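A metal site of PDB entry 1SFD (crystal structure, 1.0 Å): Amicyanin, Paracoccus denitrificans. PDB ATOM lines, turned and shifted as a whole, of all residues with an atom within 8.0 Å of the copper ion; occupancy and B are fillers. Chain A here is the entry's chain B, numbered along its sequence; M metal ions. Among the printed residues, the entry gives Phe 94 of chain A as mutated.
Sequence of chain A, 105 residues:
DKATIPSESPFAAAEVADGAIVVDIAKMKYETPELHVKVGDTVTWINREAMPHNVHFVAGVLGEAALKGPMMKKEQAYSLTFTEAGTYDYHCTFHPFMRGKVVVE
NE2 of His 53 sits close to O of Met 51 (3.4 Å).
A ring nitrogen (NE2) of His 53 sits at hydrogen-bond distance from the side-chain carboxylate (OE2) of Glu 49, 2.7 Å away.
The backbone NH (N) of Met 72 sits at hydrogen-bond distance from the backbone carbonyl oxygen (O) of His 53 (2.8 Å).
A ring nitrogen (NE2) of His 95 lies within hydrogen-bond range of the side-chain sulfur of Met 51, 3.5 Å away.
The side-chain sulfur (SG) of Cys 92 sits close to the backbone NH (N) of Phe 94, 3.6 Å away.
The backbone NH of Asn 54 sits close to the side-chain sulfur of Cys 92, 3.6 Å away.
The side-chain hydroxyl of Tyr 30 lies within hydrogen-bond range of the backbone NH of Cys 92.
O of Pro 52 touches the copper ion (3.8 Å).
Five residues have an atom within 4 Å of the copper ion: Pro 52, His 53, Cys 92, His 95 and Met 98.
Along chain A the residues within 4 Å of the copper ion span positions 52 to 98.
The nearest printed residue that does not touch the copper ion is Phe 94 (4.4 Å).
The copper ion is bound by a ring nitrogen (ND1) of His 53 (2.0 Å), a ring nitrogen (ND1) of His 95 (2.0 Å), the side-chain sulfur (SG) of Cys 92 (2.2 Å) and the side-chain sulfur (SD) of Met 98 (2.7 Å).
The copper ion has four donor atoms within binding distance.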
ATOM      1  N   ILE A  25       1.758 -37.649   5.846  1.00  0.00           N
ATOM      2  CA  ILE A  25       1.189 -36.340   5.645  1.00  0.00           C
ATOM      3  C   ILE A  25      -0.204 -36.521   5.043  1.00  0.00           C
ATOM      4  O   ILE A  25      -0.364 -37.173   4.016  1.00  0.00           O
ATOM      5  CB  ILE A  25       2.072 -35.437   4.755  1.00  0.00           C
ATOM      6  CG1 ILE A  25       3.551 -35.557   5.039  1.00  0.00           C
ATOM      7  CG2 ILE A  25       1.562 -34.007   4.856  1.00  0.00           C
ATOM      8  CD1 ILE A  25       4.474 -34.875   4.024  1.00  0.00           C
ATOM      9  N   MET A  28      -3.651 -31.933   5.402  1.00  0.00           N
ATOM     10  CA  MET A  28      -2.897 -30.725   5.647  1.00  0.00           C
ATOM     11  C   MET A  28      -2.099 -30.761   6.930  1.00  0.00           C
ATOM     12  O   MET A  28      -1.825 -29.694   7.508  1.00  0.00           O
ATOM     13  CB  MET A  28      -3.795 -29.454   5.607  1.00  0.00           C
ATOM     14  CG  MET A  28      -4.615 -29.333   4.348  1.00  0.00           C
ATOM     15  SD  MET A  28      -3.711 -29.296   2.802  1.00  0.00           S
ATOM     16  CE  MET A  28      -2.948 -27.698   2.927  1.00  0.00           C
ATOM     17  N   LYS A  29      -1.677 -31.958   7.385  1.00  0.00           N
ATOM     18  CA  LYS A  29      -0.967 -32.087   8.659  1.00  0.00           C
ATOM     19  C   LYS A  29       0.106 -33.147   8.576  1.00  0.00           C
ATOM     20  O   LYS A  29      -0.083 -34.162   7.882  1.00  0.00           O
ATOM     21  CB  LYS A  29      -1.928 -32.517   9.780  1.00  0.00           C
ATOM     22  CG  LYS A  29      -3.078 -31.579  10.016  1.00  0.00           C
ATOM     23  CD  LYS A  29      -4.042 -32.136  11.069  1.00  0.00           C
ATOM     24  CE  LYS A  29      -5.438 -31.500  10.951  1.00  0.00           C
ATOM     25  NZ  LYS A  29      -6.163 -32.127   9.803  1.00  0.00           N
ATOM     26  N   TYR A  30       1.198 -32.949   9.282  1.00  0.00           N
ATOM     27  CA  TYR A  30       2.111 -34.046   9.556  1.00  0.00           C
ATOM     28  C   TYR A  30       1.499 -34.884  10.669  1.00  0.00           C
ATOM     29  O   TYR A  30       1.153 -34.399  11.737  1.00  0.00           O
ATOM     30  CB  TYR A  30       3.459 -33.463  10.011  1.00  0.00           C
ATOM     31  CG  TYR A  30       4.100 -32.542   8.994  1.00  0.00           C
ATOM     32  CD1 TYR A  30       4.590 -33.030   7.789  1.00  0.00           C
ATOM     33  CD2 TYR A  30       4.227 -31.178   9.238  1.00  0.00           C
ATOM     34  CE1 TYR A  30       5.165 -32.191   6.847  1.00  0.00           C
ATOM     35  CE2 TYR A  30       4.817 -30.335   8.329  1.00  0.00           C
ATOM     36  CZ  TYR A  30       5.300 -30.842   7.124  1.00  0.00           C
ATOM     37  OH  TYR A  30       5.908 -29.964   6.280  1.00  0.00           O
ATOM     38  N   ASN A  47       3.924 -38.452   1.674  1.00  0.00           N
ATOM     39  CA  ASN A  47       2.705 -37.715   1.401  1.00  0.00           C
ATOM     40  C   ASN A  47       1.618 -38.724   1.008  1.00  0.00           C
ATOM     41  O   ASN A  47       1.724 -39.457   0.042  1.00  0.00           O
ATOM     42  CB  ASN A  47       2.902 -36.701   0.250  1.00  0.00           C
ATOM     43  CG  ASN A  47       1.688 -35.827   0.117  1.00  0.00           C
ATOM     44  OD1 ASN A  47       0.729 -35.936   0.898  1.00  0.00           O
ATOM     45  ND2 ASN A  47       1.670 -34.943  -0.847  1.00  0.00           N
ATOM     46  N   GLU A  49      -1.642 -37.814   0.497  1.00  0.00           N
ATOM     47  CA  GLU A  49      -2.788 -37.134  -0.093  1.00  0.00           C
ATOM     48  C   GLU A  49      -2.403 -36.436  -1.406  1.00  0.00           C
ATOM     49  O   GLU A  49      -1.250 -36.243  -1.750  1.00  0.00           O
ATOM     50  CB  GLU A  49      -3.433 -36.174   0.887  1.00  0.00           C
ATOM     51  CG  GLU A  49      -2.617 -34.963   1.295  1.00  0.00           C
ATOM     52  CD  GLU A  49      -3.375 -34.008   2.176  1.00  0.00           C
ATOM     53  OE1 GLU A  49      -4.601 -34.143   2.249  1.00  0.00           O
ATOM     54  OE2 GLU A  49      -2.774 -33.112   2.806  1.00  0.00           O
ATOM     55  N   MET A  51      -2.892 -33.258  -2.297  1.00  0.00           N
ATOM     56  CA  MET A  51      -2.242 -31.963  -2.094  1.00  0.00           C
ATOM     57  C   MET A  51      -0.727 -32.182  -1.945  1.00  0.00           C
ATOM     58  O   MET A  51      -0.329 -32.921  -1.062  1.00  0.00           O
ATOM     59  CB  MET A  51      -2.748 -31.316  -0.831  1.00  0.00           C
ATOM     60  CG  MET A  51      -2.046 -30.035  -0.443  1.00  0.00           C
ATOM     61  SD  MET A  51      -2.261 -28.705  -1.679  1.00  0.00           S
ATOM     62  CE  MET A  51      -3.882 -28.158  -1.211  1.00  0.00           C
ATOM     63  N   PRO A  52       0.096 -31.494  -2.758  1.00  0.00           N
ATOM     64  CA  PRO A  52       1.555 -31.626  -2.558  1.00  0.00           C
ATOM     65  C   PRO A  52       2.032 -30.940  -1.281  1.00  0.00           C
ATOM     66  O   PRO A  52       1.477 -29.954  -0.837  1.00  0.00           O
ATOM     67  CB  PRO A  52       2.134 -30.924  -3.792  1.00  0.00           C
ATOM     68  CG  PRO A  52       1.032 -31.047  -4.806  1.00  0.00           C
ATOM     69  CD  PRO A  52      -0.238 -30.733  -3.972  1.00  0.00           C
ATOM     70  N   HIS A  53       3.137 -31.493  -0.740  1.00  0.00           N
ATOM     71  CA  HIS A  53       3.743 -30.991   0.473  1.00  0.00           C
ATOM     72  C   HIS A  53       5.256 -31.130   0.392  1.00  0.00           C
ATOM     73  O   HIS A  53       5.762 -31.870  -0.455  1.00  0.00           O
ATOM     74  CB  HIS A  53       3.241 -31.714   1.716  1.00  0.00           C
ATOM     75  CG  HIS A  53       1.777 -31.599   1.945  1.00  0.00           C
ATOM     76  ND1 HIS A  53       1.171 -30.417   2.342  1.00  0.00           N
ATOM     77  CD2 HIS A  53       0.816 -32.559   1.831  1.00  0.00           C
ATOM     78  CE1 HIS A  53      -0.132 -30.672   2.481  1.00  0.00           C
ATOM     79  NE2 HIS A  53      -0.385 -31.971   2.160  1.00  0.00           N
ATOM     80  N   ASN A  54       5.989 -30.522   1.294  1.00  0.00           N
ATOM     81  CA  ASN A  54       7.400 -30.830   1.508  1.00  0.00           C
ATOM     82  C   ASN A  54       7.717 -30.764   2.987  1.00  0.00           C
ATOM     83  O   ASN A  54       6.799 -30.609   3.812  1.00  0.00           O
ATOM     84  CB  ASN A  54       8.350 -29.967   0.647  1.00  0.00           C
ATOM     85  CG  ASN A  54       8.478 -28.555   1.211  1.00  0.00           C
ATOM     86  OD1 ASN A  54       7.671 -28.131   2.027  1.00  0.00           O
ATOM     87  ND2 ASN A  54       9.550 -27.902   0.731  1.00  0.00           N
ATOM     88  N   VAL A  55       8.986 -30.873   3.325  1.00  0.00           N
ATOM     89  CA  VAL A  55       9.501 -30.486   4.643  1.00  0.00           C
ATOM     90  C   VAL A  55      10.581 -29.451   4.437  1.00  0.00           C
ATOM     91  O   VAL A  55      11.374 -29.540   3.500  1.00  0.00           O
ATOM     92  CB  VAL A  55       9.999 -31.700   5.458  1.00  0.00           C
ATOM     93  CG1 VAL A  55       8.843 -32.640   5.798  1.00  0.00           C
ATOM     94  CG2 VAL A  55      11.137 -32.407   4.762  1.00  0.00           C
ATOM     95  N   MET A  72       6.715 -33.174  -2.772  1.00  0.00           N
ATOM     96  CA  MET A  72       6.232 -34.534  -2.726  1.00  0.00           C
ATOM     97  C   MET A  72       4.780 -34.585  -3.143  1.00  0.00           C
ATOM     98  O   MET A  72       3.928 -33.999  -2.472  1.00  0.00           O
ATOM     99  CB  MET A  72       6.339 -35.073  -1.301  1.00  0.00           C
ATOM    100  CG  MET A  72       7.774 -34.746  -0.758  1.00  0.00           C
ATOM    101  SD  MET A  72       7.878 -34.879   1.073  1.00  0.00           S
ATOM    102  CE  MET A  72       7.483 -36.396   1.158  1.00  0.00           C
ATOM    103  N   HIS A  91       8.585 -27.004   8.662  1.00  0.00           N
ATOM    104  CA  HIS A  91       7.263 -26.599   8.163  1.00  0.00           C
ATOM    105  C   HIS A  91       7.178 -26.991   6.701  1.00  0.00           C
ATOM    106  O   HIS A  91       8.137 -27.461   6.095  1.00  0.00           O
ATOM    107  CB  HIS A  91       7.026 -25.080   8.359  1.00  0.00           C
ATOM    108  CG  HIS A  91       7.897 -24.237   7.502  1.00  0.00           C
ATOM    109  ND1 HIS A  91       9.197 -23.903   7.843  1.00  0.00           N
ATOM    110  CD2 HIS A  91       7.634 -23.680   6.289  1.00  0.00           C
ATOM    111  CE1 HIS A  91       9.695 -23.118   6.865  1.00  0.00           C
ATOM    112  NE2 HIS A  91       8.783 -22.996   5.900  1.00  0.00           N
ATOM    113  N   CYS A  92       6.014 -26.781   6.111  1.00  0.00           N
ATOM    114  CA  CYS A  92       5.791 -27.018   4.690  1.00  0.00           C
ATOM    115  C   CYS A  92       5.938 -25.687   3.939  1.00  0.00           C
ATOM    116  O   CYS A  92       5.263 -24.702   4.279  1.00  0.00           O
ATOM    117  CB  CYS A  92       4.396 -27.575   4.466  1.00  0.00           C
ATOM    118  SG  CYS A  92       4.042 -27.892   2.721  1.00  0.00           S
ATOM    119  N   THR A  93       6.805 -25.633   2.952  1.00  0.00           N
ATOM    120  CA  THR A  93       6.980 -24.378   2.190  1.00  0.00           C
ATOM    121  C   THR A  93       5.672 -23.912   1.586  1.00  0.00           C
ATOM    122  O   THR A  93       5.365 -22.727   1.529  1.00  0.00           O
ATOM    123  CB  THR A  93       8.004 -24.605   1.049  1.00  0.00           C
ATOM    124  OG1 THR A  93       9.238 -25.051   1.623  1.00  0.00           O
ATOM    125  CG2 THR A  93       8.221 -23.368   0.257  1.00  0.00           C
ATOM    126  N   PHE A  94       4.890 -24.874   1.050  1.00  0.00           N
ATOM    127  CA  PHE A  94       3.661 -24.494   0.398  1.00  0.00           C
ATOM    128  C   PHE A  94       2.637 -23.981   1.354  1.00  0.00           C
ATOM    129  O   PHE A  94       1.789 -23.106   1.009  1.00  0.00           O
ATOM    130  CB  PHE A  94       3.106 -25.710  -0.387  1.00  0.00           C
ATOM    131  CG  PHE A  94       4.103 -26.342  -1.306  1.00  0.00           C
ATOM    132  CD1 PHE A  94       4.508 -27.625  -1.086  1.00  0.00           C
ATOM    133  CD2 PHE A  94       4.600 -25.696  -2.397  1.00  0.00           C
ATOM    134  CE1 PHE A  94       5.400 -28.236  -1.945  1.00  0.00           C
ATOM    135  CE2 PHE A  94       5.504 -26.278  -3.255  1.00  0.00           C
ATOM    136  CZ  PHE A  94       5.909 -27.573  -3.007  1.00  0.00           C
ATOM    137  N   HIS A  95       2.637 -24.569   2.561  1.00  0.00           N
ATOM    138  CA  HIS A  95       1.627 -24.346   3.578  1.00  0.00           C
ATOM    139  C   HIS A  95       2.324 -24.069   4.910  1.00  0.00           C
ATOM    140  O   HIS A  95       2.448 -24.995   5.747  1.00  0.00           O
ATOM    141  CB  HIS A  95       0.689 -25.570   3.718  1.00  0.00           C
ATOM    142  CG  HIS A  95       0.234 -26.080   2.374  1.00  0.00           C
ATOM    143  ND1 HIS A  95       0.605 -27.324   1.900  1.00  0.00           N
ATOM    144  CD2 HIS A  95      -0.524 -25.491   1.439  1.00  0.00           C
ATOM    145  CE1 HIS A  95       0.067 -27.465   0.700  1.00  0.00           C
ATOM    146  NE2 HIS A  95      -0.633 -26.369   0.357  1.00  0.00           N
ATOM    147  N   PRO A  96       2.834 -22.867   5.154  1.00  0.00           N
ATOM    148  CA  PRO A  96       3.716 -22.664   6.309  1.00  0.00           C
ATOM    149  C   PRO A  96       3.096 -22.884   7.661  1.00  0.00           C
ATOM    150  O   PRO A  96       3.773 -23.091   8.639  1.00  0.00           O
ATOM    151  CB  PRO A  96       4.213 -21.231   6.130  1.00  0.00           C
ATOM    152  CG  PRO A  96       4.209 -21.081   4.629  1.00  0.00           C
ATOM    153  CD  PRO A  96       2.924 -21.735   4.208  1.00  0.00           C
ATOM    154  N   PHE A  97       1.759 -22.906   7.716  1.00  0.00           N
ATOM    155  CA  PHE A  97       1.030 -23.251   8.931  1.00  0.00           C
ATOM    156  C   PHE A  97       1.242 -24.716   9.316  1.00  0.00           C
ATOM    157  O   PHE A  97       0.928 -25.061  10.461  1.00  0.00           O
ATOM    158  CB  PHE A  97      -0.456 -22.913   8.795  1.00  0.00           C
ATOM    159  CG  PHE A  97      -1.161 -23.614   7.666  1.00  0.00           C
ATOM    160  CD1 PHE A  97      -1.591 -24.944   7.764  1.00  0.00           C
ATOM    161  CD2 PHE A  97      -1.437 -22.932   6.473  1.00  0.00           C
ATOM    162  CE1 PHE A  97      -2.241 -25.594   6.732  1.00  0.00           C
ATOM    163  CE2 PHE A  97      -2.063 -23.581   5.444  1.00  0.00           C
ATOM    164  CZ  PHE A  97      -2.490 -24.880   5.573  1.00  0.00           C
ATOM    165  N   MET A  98       1.645 -25.574   8.395  1.00  0.00           N
ATOM    166  CA  MET A  98       1.920 -26.988   8.675  1.00  0.00           C
ATOM    167  C   MET A  98       3.264 -27.071   9.399  1.00  0.00           C
ATOM    168  O   MET A  98       4.279 -26.696   8.818  1.00  0.00           O
ATOM    169  CB  MET A  98       1.974 -27.801   7.402  1.00  0.00           C
ATOM    170  CG  MET A  98       0.688 -27.906   6.654  1.00  0.00           C
ATOM    171  SD  MET A  98       0.745 -28.911   5.163  1.00  0.00           S
ATOM    172  CE  MET A  98       1.405 -30.473   5.796  1.00  0.00           C
HETATM  173 CU    CU M   1       1.943 -28.622   2.740  1.00  0.00          CU
